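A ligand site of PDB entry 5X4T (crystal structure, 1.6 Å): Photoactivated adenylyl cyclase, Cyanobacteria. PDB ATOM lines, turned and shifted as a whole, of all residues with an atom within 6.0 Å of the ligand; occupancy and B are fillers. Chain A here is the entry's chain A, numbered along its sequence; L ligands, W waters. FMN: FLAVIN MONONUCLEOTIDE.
The side-chain carboxylate (OD2) of Asp 67 is in hydrogen-bond range of an oxygen (O2') of the ligand.
OG of Ser 26 lies close to N5 of the ligand, 3.2 Å away.
O2' of the ligand sits at hydrogen-bond distance from O of Arg 63, 3.4 Å away.
The side-chain amino group (NZ) of Lys 29 lies within salt-bridge range of an oxygen (O1P) of the ligand.
A nitrogen (N3) of the ligand is in hydrogen-bond range of the side-chain amide oxygen (OD1) of Asn 30 (2.8 Å).
The guanidinium group (NE) of Arg 63 lies within salt-bridge range of an oxygen (O1P) of the ligand (3.9 Å).
An oxygen (O4) of the ligand is in hydrogen-bond range of the side-chain amide nitrogen (NE2) of Gln 48, at 2.6 Å.
NH2 of Arg 69 lies within hydrogen-bond range of O3' of the ligand, 3.5 Å away.
The backbone NH (N) of Val 35 sits at hydrogen-bond distance from the backbone carbonyl oxygen (O) of Asn 30 (2.8 Å).
The backbone carbonyl oxygen (O) of Ser 8 lies within hydrogen-bond range of the backbone NH (N) of Phe 46, 2.8 Å away.
The side-chain hydroxyl (OG) of Ser 26 sits at hydrogen-bond distance from the backbone carbonyl oxygen (O) of Ile 22 (2.7 Å).
The side-chain amide nitrogen (ND2) of Asn 30 lies close to the backbone carbonyl oxygen (O) of Ser 26 (3.4 Å).
The side-chain sulfur of Met 92 lies within hydrogen-bond range of the backbone NH of Leu 39 (3.7 Å).
The side-chain hydroxyl (OG) of Ser 8 sits at hydrogen-bond distance from a ring nitrogen (ND1) of His 70, at 2.7 Å.
The guanidinium group (NH2) of Arg 69 lies within salt-bridge range of the side-chain carboxylate (OD2) of Asp 67 (2.7 Å).
The side-chain sulfur (SD) of Met 92 lies close to the side-chain amide nitrogen (NE2) of Gln 48, 3.3 Å away.
Residues that only touch the ligand: Tyr 6 (3.3 Å), Ile 22 (3.7 Å), Phe 46 (3.5 Å), Leu 50 (3.5 Å), Ile 60 (3.4 Å), Ile 64 (3.6 Å), His 70 (3.7 Å) and Met 92 (3.98 Å).
Hydrophobic or aromatic side chains that line the ligand: Ile 22, Phe 46, Leu 50, Ile 60, Ile 64, His 70 and Met 92.
Within 4 Å of the ligand: Tyr 6, Ile 22, Ser 26, Lys 29, Asn 30, Phe 46, Gln 48, Leu 50, Ile 60, Arg 63, Ile 64, Asp 67, Arg 69, His 70 and Met 92.
Along chain A the residues within 4 Å of the ligand span positions 6 to 92.
Water W2 lies within hydrogen-bond range of O3' of the ligand (2.7 Å) and OD2 of Asp 67 (3.1 Å).
Water W1 lies within hydrogen-bond range of O3' of the ligand and NH2 of Arg 69.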
ATOM      1  N   TYR A   6      21.951 -22.203  -3.127  1.00  0.00           N
ATOM      2  CA  TYR A   6      22.872 -22.023  -4.236  1.00  0.00           C
ATOM      3  C   TYR A   6      23.750 -20.812  -3.978  1.00  0.00           C
ATOM      4  O   TYR A   6      23.483 -19.980  -3.113  1.00  0.00           O
ATOM      5  CB  TYR A   6      22.133 -21.853  -5.589  1.00  0.00           C
ATOM      6  CG  TYR A   6      21.475 -20.485  -5.755  1.00  0.00           C
ATOM      7  CD1 TYR A   6      22.203 -19.392  -6.237  1.00  0.00           C
ATOM      8  CD2 TYR A   6      20.143 -20.273  -5.397  1.00  0.00           C
ATOM      9  CE1 TYR A   6      21.629 -18.143  -6.363  1.00  0.00           C
ATOM     10  CE2 TYR A   6      19.555 -19.029  -5.539  1.00  0.00           C
ATOM     11  CZ  TYR A   6      20.299 -17.965  -6.013  1.00  0.00           C
ATOM     12  OH  TYR A   6      19.734 -16.717  -6.134  1.00  0.00           O
ATOM     13  N   SER A   8      26.130 -17.798  -6.349  1.00  0.00           N
ATOM     14  CA  SER A   8      26.309 -17.236  -7.688  1.00  0.00           C
ATOM     15  C   SER A   8      27.251 -16.042  -7.607  1.00  0.00           C
ATOM     16  O   SER A   8      27.543 -15.522  -6.523  1.00  0.00           O
ATOM     17  CB  SER A   8      24.980 -16.827  -8.304  1.00  0.00           C
ATOM     18  OG  SER A   8      24.468 -15.677  -7.640  1.00  0.00           O
ATOM     19  N   ILE A  22      16.452  -6.184  -6.234  1.00  0.00           N
ATOM     20  CA  ILE A  22      16.338  -7.640  -6.281  1.00  0.00           C
ATOM     21  C   ILE A  22      15.615  -8.147  -5.031  1.00  0.00           C
ATOM     22  O   ILE A  22      14.701  -8.972  -5.121  1.00  0.00           O
ATOM     23  CB  ILE A  22      17.722  -8.288  -6.435  1.00  0.00           C
ATOM     24  CG1 ILE A  22      18.335  -7.940  -7.792  1.00  0.00           C
ATOM     25  CG2 ILE A  22      17.641  -9.808  -6.205  1.00  0.00           C
ATOM     26  CD1 ILE A  22      19.814  -8.308  -7.921  1.00  0.00           C
ATOM     27  N   ILE A  25      11.707  -7.234  -5.234  1.00  0.00           N
ATOM     28  CA  ILE A  25      10.894  -8.079  -6.108  1.00  0.00           C
ATOM     29  C   ILE A  25      10.882  -9.508  -5.605  1.00  0.00           C
ATOM     30  O   ILE A  25       9.830 -10.166  -5.615  1.00  0.00           O
ATOM     31  CB  ILE A  25      11.404  -7.991  -7.558  1.00  0.00           C
ATOM     32  CG1 ILE A  25      11.160  -6.587  -8.121  1.00  0.00           C
ATOM     33  CG2 ILE A  25      10.716  -9.044  -8.431  1.00  0.00           C
ATOM     34  CD1 ILE A  25      11.492  -6.458  -9.596  1.00  0.00           C
ATOM     35  N   SER A  26      12.031 -10.014  -5.149  1.00  0.00           N
ATOM     36  CA  SER A  26      12.100 -11.387  -4.660  1.00  0.00           C
ATOM     37  C   SER A  26      11.143 -11.600  -3.492  1.00  0.00           C
ATOM     38  O   SER A  26      10.417 -12.589  -3.444  1.00  0.00           O
ATOM     39  CB  SER A  26      13.535 -11.712  -4.240  1.00  0.00           C
ATOM     40  OG  SER A  26      14.413 -11.673  -5.350  1.00  0.00           O
ATOM     41  N   SER A  27      11.144 -10.660  -2.539  1.00  0.00           N
ATOM     42  CA  SER A  27      10.271 -10.789  -1.367  1.00  0.00           C
ATOM     43  C   SER A  27       8.802 -10.750  -1.760  1.00  0.00           C
ATOM     44  O   SER A  27       7.976 -11.485  -1.205  1.00  0.00           O
ATOM     45  CB  SER A  27      10.590  -9.689  -0.367  1.00  0.00           C
ATOM     46  OG  SER A  27       9.746  -9.759   0.760  1.00  0.00           O
ATOM     47  N   LYS A  29       7.422 -11.635  -4.695  1.00  0.00           N
ATOM     48  CA  LYS A  29       7.013 -12.841  -5.410  1.00  0.00           C
ATOM     49  C   LYS A  29       7.054 -14.068  -4.511  1.00  0.00           C
ATOM     50  O   LYS A  29       6.188 -14.950  -4.610  1.00  0.00           O
ATOM     51  CB  LYS A  29       7.888 -13.024  -6.659  1.00  0.00           C
ATOM     52  CG  LYS A  29       7.624 -11.965  -7.714  1.00  0.00           C
ATOM     53  CD  LYS A  29       8.299 -12.304  -9.015  1.00  0.00           C
ATOM     54  CE  LYS A  29       7.598 -11.603 -10.172  1.00  0.00           C
ATOM     55  NZ  LYS A  29       6.206 -12.101 -10.336  1.00  0.00           N
ATOM     56  N   ASN A  30       8.037 -14.151  -3.616  1.00  0.00           N
ATOM     57  CA  ASN A  30       8.064 -15.293  -2.703  1.00  0.00           C
ATOM     58  C   ASN A  30       6.904 -15.261  -1.718  1.00  0.00           C
ATOM     59  O   ASN A  30       6.377 -16.315  -1.339  1.00  0.00           O
ATOM     60  CB  ASN A  30       9.390 -15.350  -1.961  1.00  0.00           C
ATOM     61  CG  ASN A  30      10.557 -15.680  -2.871  1.00  0.00           C
ATOM     62  OD1 ASN A  30      10.368 -16.083  -4.020  1.00  0.00           O
ATOM     63  ND2 ASN A  30      11.765 -15.503  -2.361  1.00  0.00           N
ATOM     64  N   VAL A  35       6.891 -18.869  -0.288  1.00  0.00           N
ATOM     65  CA  VAL A  35       8.295 -19.291  -0.251  1.00  0.00           C
ATOM     66  C   VAL A  35       9.023 -18.412   0.757  1.00  0.00           C
ATOM     67  O   VAL A  35       8.782 -17.202   0.853  1.00  0.00           O
ATOM     68  CB  VAL A  35       8.929 -19.202  -1.654  1.00  0.00           C
ATOM     69  CG1 VAL A  35      10.474 -19.233  -1.576  1.00  0.00           C
ATOM     70  CG2 VAL A  35       8.423 -20.336  -2.534  1.00  0.00           C
ATOM     71  N   LEU A  39      18.499 -14.253   1.300  1.00  0.00           N
ATOM     72  CA  LEU A  39      19.434 -13.920   0.226  1.00  0.00           C
ATOM     73  C   LEU A  39      20.541 -13.060   0.830  1.00  0.00           C
ATOM     74  O   LEU A  39      20.264 -12.016   1.433  1.00  0.00           O
ATOM     75  CB  LEU A  39      18.724 -13.171  -0.909  1.00  0.00           C
ATOM     76  CG  LEU A  39      19.632 -12.541  -1.963  1.00  0.00           C
ATOM     77  CD1 LEU A  39      20.378 -13.626  -2.708  1.00  0.00           C
ATOM     78  CD2 LEU A  39      18.804 -11.711  -2.924  1.00  0.00           C
ATOM     79  N   PHE A  46      26.540 -13.884  -4.418  1.00  0.00           N
ATOM     80  CA  PHE A  46      25.226 -14.136  -3.842  1.00  0.00           C
ATOM     81  C   PHE A  46      25.180 -15.519  -3.192  1.00  0.00           C
ATOM     82  O   PHE A  46      25.790 -16.471  -3.704  1.00  0.00           O
ATOM     83  CB  PHE A  46      24.121 -14.081  -4.891  1.00  0.00           C
ATOM     84  CG  PHE A  46      23.801 -12.695  -5.384  1.00  0.00           C
ATOM     85  CD1 PHE A  46      23.332 -11.732  -4.513  1.00  0.00           C
ATOM     86  CD2 PHE A  46      23.956 -12.367  -6.729  1.00  0.00           C
ATOM     87  CE1 PHE A  46      23.007 -10.464  -4.951  1.00  0.00           C
ATOM     88  CE2 PHE A  46      23.629 -11.098  -7.184  1.00  0.00           C
ATOM     89  CZ  PHE A  46      23.165 -10.142  -6.302  1.00  0.00           C
ATOM     90  N   GLN A  48      21.867 -17.922  -1.603  1.00  0.00           N
ATOM     91  CA  GLN A  48      20.433 -17.913  -1.333  1.00  0.00           C
ATOM     92  C   GLN A  48      19.933 -19.289  -0.918  1.00  0.00           C
ATOM     93  O   GLN A  48      20.315 -20.302  -1.500  1.00  0.00           O
ATOM     94  CB  GLN A  48      19.622 -17.426  -2.543  1.00  0.00           C
ATOM     95  CG  GLN A  48      18.179 -17.129  -2.144  1.00  0.00           C
ATOM     96  CD  GLN A  48      17.270 -16.633  -3.264  1.00  0.00           C
ATOM     97  OE1 GLN A  48      17.674 -16.488  -4.419  1.00  0.00           O
ATOM     98  NE2 GLN A  48      16.030 -16.338  -2.896  1.00  0.00           N
ATOM     99  N   LEU A  50      16.139 -21.059  -0.414  1.00  0.00           N
ATOM    100  CA  LEU A  50      14.722 -20.885  -0.720  1.00  0.00           C
ATOM    101  C   LEU A  50      14.002 -22.175  -0.353  1.00  0.00           C
ATOM    102  O   LEU A  50      14.487 -23.261  -0.660  1.00  0.00           O
ATOM    103  CB  LEU A  50      14.453 -20.594  -2.195  1.00  0.00           C
ATOM    104  CG  LEU A  50      15.244 -19.603  -3.023  1.00  0.00           C
ATOM    105  CD1 LEU A  50      16.544 -20.232  -3.493  1.00  0.00           C
ATOM    106  CD2 LEU A  50      14.390 -19.195  -4.207  1.00  0.00           C
ATOM    107  N   ILE A  60      10.535 -20.711  -9.506  1.00  0.00           N
ATOM    108  CA  ILE A  60      11.347 -19.585  -9.063  1.00  0.00           C
ATOM    109  C   ILE A  60      12.804 -19.791  -9.456  1.00  0.00           C
ATOM    110  O   ILE A  60      13.440 -18.907 -10.045  1.00  0.00           O
ATOM    111  CB  ILE A  60      11.208 -19.388  -7.545  1.00  0.00           C
ATOM    112  CG1 ILE A  60       9.787 -18.931  -7.205  1.00  0.00           C
ATOM    113  CG2 ILE A  60      12.247 -18.400  -7.030  1.00  0.00           C
ATOM    114  CD1 ILE A  60       9.484 -18.996  -5.733  1.00  0.00           C
ATOM    115  N   ARG A  63      13.491 -19.069 -13.082  1.00  0.00           N
ATOM    116  CA  ARG A  63      13.697 -17.647 -13.361  1.00  0.00           C
ATOM    117  C   ARG A  63      15.055 -17.175 -12.859  1.00  0.00           C
ATOM    118  O   ARG A  63      15.749 -16.419 -13.562  1.00  0.00           O
ATOM    119  CB  ARG A  63      12.588 -16.809 -12.718  1.00  0.00           C
ATOM    120  CG  ARG A  63      11.184 -17.183 -13.191  1.00  0.00           C
ATOM    121  CD  ARG A  63      10.216 -16.052 -12.962  1.00  0.00           C
ATOM    122  NE  ARG A  63      10.003 -15.761 -11.546  1.00  0.00           N
ATOM    123  CZ  ARG A  63       9.138 -16.420 -10.772  1.00  0.00           C
ATOM    124  NH1 ARG A  63       8.986 -16.076  -9.496  1.00  0.00           N
ATOM    125  NH2 ARG A  63       8.423 -17.408 -11.289  1.00  0.00           N
ATOM    126  N   ILE A  64      15.433 -17.582 -11.647  1.00  0.00           N
ATOM    127  CA  ILE A  64      16.741 -17.205 -11.107  1.00  0.00           C
ATOM    128  C   ILE A  64      17.854 -17.643 -12.056  1.00  0.00           C
ATOM    129  O   ILE A  64      18.784 -16.881 -12.345  1.00  0.00           O
ATOM    130  CB  ILE A  64      16.930 -17.780  -9.687  1.00  0.00           C
ATOM    131  CG1 ILE A  64      15.924 -17.167  -8.723  1.00  0.00           C
ATOM    132  CG2 ILE A  64      18.351 -17.535  -9.197  1.00  0.00           C
ATOM    133  CD1 ILE A  64      15.992 -17.741  -7.291  1.00  0.00           C
ATOM    134  N   LEU A  65      17.755 -18.878 -12.570  1.00  0.00           N
ATOM    135  CA  LEU A  65      18.772 -19.403 -13.482  1.00  0.00           C
ATOM    136  C   LEU A  65      18.900 -18.570 -14.742  1.00  0.00           C
ATOM    137  O   LEU A  65      19.989 -18.512 -15.330  1.00  0.00           O
ATOM    138  CB  LEU A  65      18.426 -20.850 -13.849  1.00  0.00           C
ATOM    139  CG  LEU A  65      18.773 -21.916 -12.821  1.00  0.00           C
ATOM    140  CD1 LEU A  65      18.371 -23.288 -13.322  1.00  0.00           C
ATOM    141  CD2 LEU A  65      20.247 -21.872 -12.509  1.00  0.00           C
ATOM    142  N   ALA A  66      17.815 -17.945 -15.195  1.00  0.00           N
ATOM    143  CA  ALA A  66      17.815 -17.141 -16.416  1.00  0.00           C
ATOM    144  C   ALA A  66      18.166 -15.684 -16.176  1.00  0.00           C
ATOM    145  O   ALA A  66      18.275 -14.923 -17.150  1.00  0.00           O
ATOM    146  CB  ALA A  66      16.452 -17.229 -17.109  1.00  0.00           C
ATOM    147  N   ASP A  67      18.324 -15.259 -14.930  1.00  0.00           N
ATOM    148  CA  ASP A  67      18.561 -13.855 -14.620  1.00  0.00           C
ATOM    149  C   ASP A  67      19.998 -13.487 -14.994  1.00  0.00           C
ATOM    150  O   ASP A  67      20.959 -14.012 -14.435  1.00  0.00           O
ATOM    151  CB  ASP A  67      18.296 -13.596 -13.137  1.00  0.00           C
ATOM    152  CG  ASP A  67      18.108 -12.127 -12.822  1.00  0.00           C
ATOM    153  OD1 ASP A  67      18.949 -11.304 -13.232  1.00  0.00           O
ATOM    154  OD2 ASP A  67      17.116 -11.798 -12.137  1.00  0.00           O
ATOM    155  N   ARG A  69      21.691 -11.010 -14.283  1.00  0.00           N
ATOM    156  CA  ARG A  69      22.421 -10.198 -13.327  1.00  0.00           C
ATOM    157  C   ARG A  69      23.413 -11.000 -12.491  1.00  0.00           C
ATOM    158  O   ARG A  69      24.243 -10.391 -11.793  1.00  0.00           O
ATOM    159  CB  ARG A  69      21.457  -9.462 -12.404  1.00  0.00           C
ATOM    160  CG  ARG A  69      20.864  -8.228 -13.064  1.00  0.00           C
ATOM    161  CD  ARG A  69      19.739  -7.650 -12.259  1.00  0.00           C
ATOM    162  NE  ARG A  69      18.648  -8.598 -12.092  1.00  0.00           N
ATOM    163  CZ  ARG A  69      17.551  -8.330 -11.414  1.00  0.00           C
ATOM    164  NH1 ARG A  69      17.400  -7.136 -10.851  1.00  0.00           N
ATOM    165  NH2 ARG A  69      16.583  -9.241 -11.296  1.00  0.00           N
ATOM    166  N   HIS A  70      23.359 -12.330 -12.527  1.00  0.00           N
ATOM    167  CA  HIS A  70      24.399 -13.137 -11.916  1.00  0.00           C
ATOM    168  C   HIS A  70      24.710 -14.313 -12.837  1.00  0.00           C
ATOM    169  O   HIS A  70      24.021 -14.563 -13.821  1.00  0.00           O
ATOM    170  CB  HIS A  70      24.017 -13.615 -10.493  1.00  0.00           C
ATOM    171  CG  HIS A  70      22.775 -14.447 -10.412  1.00  0.00           C
ATOM    172  ND1 HIS A  70      22.370 -15.054  -9.247  1.00  0.00           N
ATOM    173  CD2 HIS A  70      21.848 -14.759 -11.350  1.00  0.00           C
ATOM    174  CE1 HIS A  70      21.250 -15.709  -9.461  1.00  0.00           C
ATOM    175  NE2 HIS A  70      20.900 -15.547 -10.729  1.00  0.00           N
ATOM    176  N   MET A  92      11.466 -13.325   1.826  1.00  0.00           N
ATOM    177  CA  MET A  92      12.812 -13.275   1.272  1.00  0.00           C
ATOM    178  C   MET A  92      13.583 -12.143   1.929  1.00  0.00           C
ATOM    179  O   MET A  92      13.734 -11.058   1.343  1.00  0.00           O
ATOM    180  CB  MET A  92      12.788 -13.093  -0.241  1.00  0.00           C
ATOM    181  CG  MET A  92      14.177 -13.127  -0.899  1.00  0.00           C
ATOM    182  SD  MET A  92      15.228 -14.465  -0.309  1.00  0.00           S
ATOM    183  CE  MET A  92      14.173 -15.906  -0.381  1.00  0.00           C
HETATM  184  N1  FMN L   1      12.880 -13.983  -7.797  1.00  0.00           N
HETATM  185  C2  FMN L   1      11.965 -14.609  -6.992  1.00  0.00           C
HETATM  186  O2  FMN L   1      10.780 -14.650  -7.325  1.00  0.00           O
HETATM  187  N3  FMN L   1      12.370 -15.198  -5.809  1.00  0.00           N
HETATM  188  C4  FMN L   1      13.699 -15.178  -5.427  1.00  0.00           C
HETATM  189  O4  FMN L   1      14.033 -15.694  -4.354  1.00  0.00           O
HETATM  190  C4A FMN L   1      14.622 -14.523  -6.242  1.00  0.00           C
HETATM  191  N5  FMN L   1      15.953 -14.466  -5.881  1.00  0.00           N
HETATM  192  C5A FMN L   1      16.867 -13.839  -6.703  1.00  0.00           C
HETATM  193  C6  FMN L   1      18.200 -13.797  -6.326  1.00  0.00           C
HETATM  194  C7  FMN L   1      19.135 -13.150  -7.142  1.00  0.00           C
HETATM  195  C7M FMN L   1      20.576 -13.121  -6.712  1.00  0.00           C
HETATM  196  C8  FMN L   1      18.729 -12.559  -8.343  1.00  0.00           C
HETATM  197  C8M FMN L   1      19.736 -11.873  -9.221  1.00  0.00           C
HETATM  198  C9  FMN L   1      17.389 -12.602  -8.708  1.00  0.00           C
HETATM  199  C9A FMN L   1      16.454 -13.235  -7.890  1.00  0.00           C
HETATM  200  N10 FMN L   1      15.117 -13.299  -8.263  1.00  0.00           N
HETATM  201  C10 FMN L   1      14.208 -13.933  -7.430  1.00  0.00           C
HETATM  202  C1' FMN L   1      14.645 -12.624  -9.520  1.00  0.00           C
HETATM  203  C2' FMN L   1      14.259 -13.490 -10.681  1.00  0.00           C
HETATM  204  O2' FMN L   1      15.459 -13.825 -11.345  1.00  0.00           O
HETATM  205  C3' FMN L   1      13.380 -12.701 -11.657  1.00  0.00           C
HETATM  206  O3' FMN L   1      13.926 -11.418 -11.880  1.00  0.00           O
HETATM  207  C4' FMN L   1      11.918 -12.512 -11.236  1.00  0.00           C
HETATM  208  O4' FMN L   1      11.520 -13.420 -10.217  1.00  0.00           O
HETATM  209  C5' FMN L   1      11.089 -12.723 -12.495  1.00  0.00           C
HETATM  210  O5' FMN L   1       9.885 -12.014 -12.446  1.00  0.00           O
HETATM  211  P   FMN L   1       8.817 -12.168 -13.643  1.00  0.00           P
HETATM  212  O1P FMN L   1       7.696 -13.082 -13.179  1.00  0.00           O
HETATM  213  O2P FMN L   1       8.264 -10.821 -14.036  1.00  0.00           O
HETATM  214  O3P FMN L   1       9.502 -12.792 -14.834  1.00  0.00           O
HETATM  215  O   HOH W   1      13.157  -8.859 -11.656  1.00  0.00           O
HETATM  216  O   HOH W   2      14.988 -11.626 -14.330  1.00  0.00           O
HETATM  217  O   HOH W   3       6.110 -15.328 -13.242  1.00  0.00           O
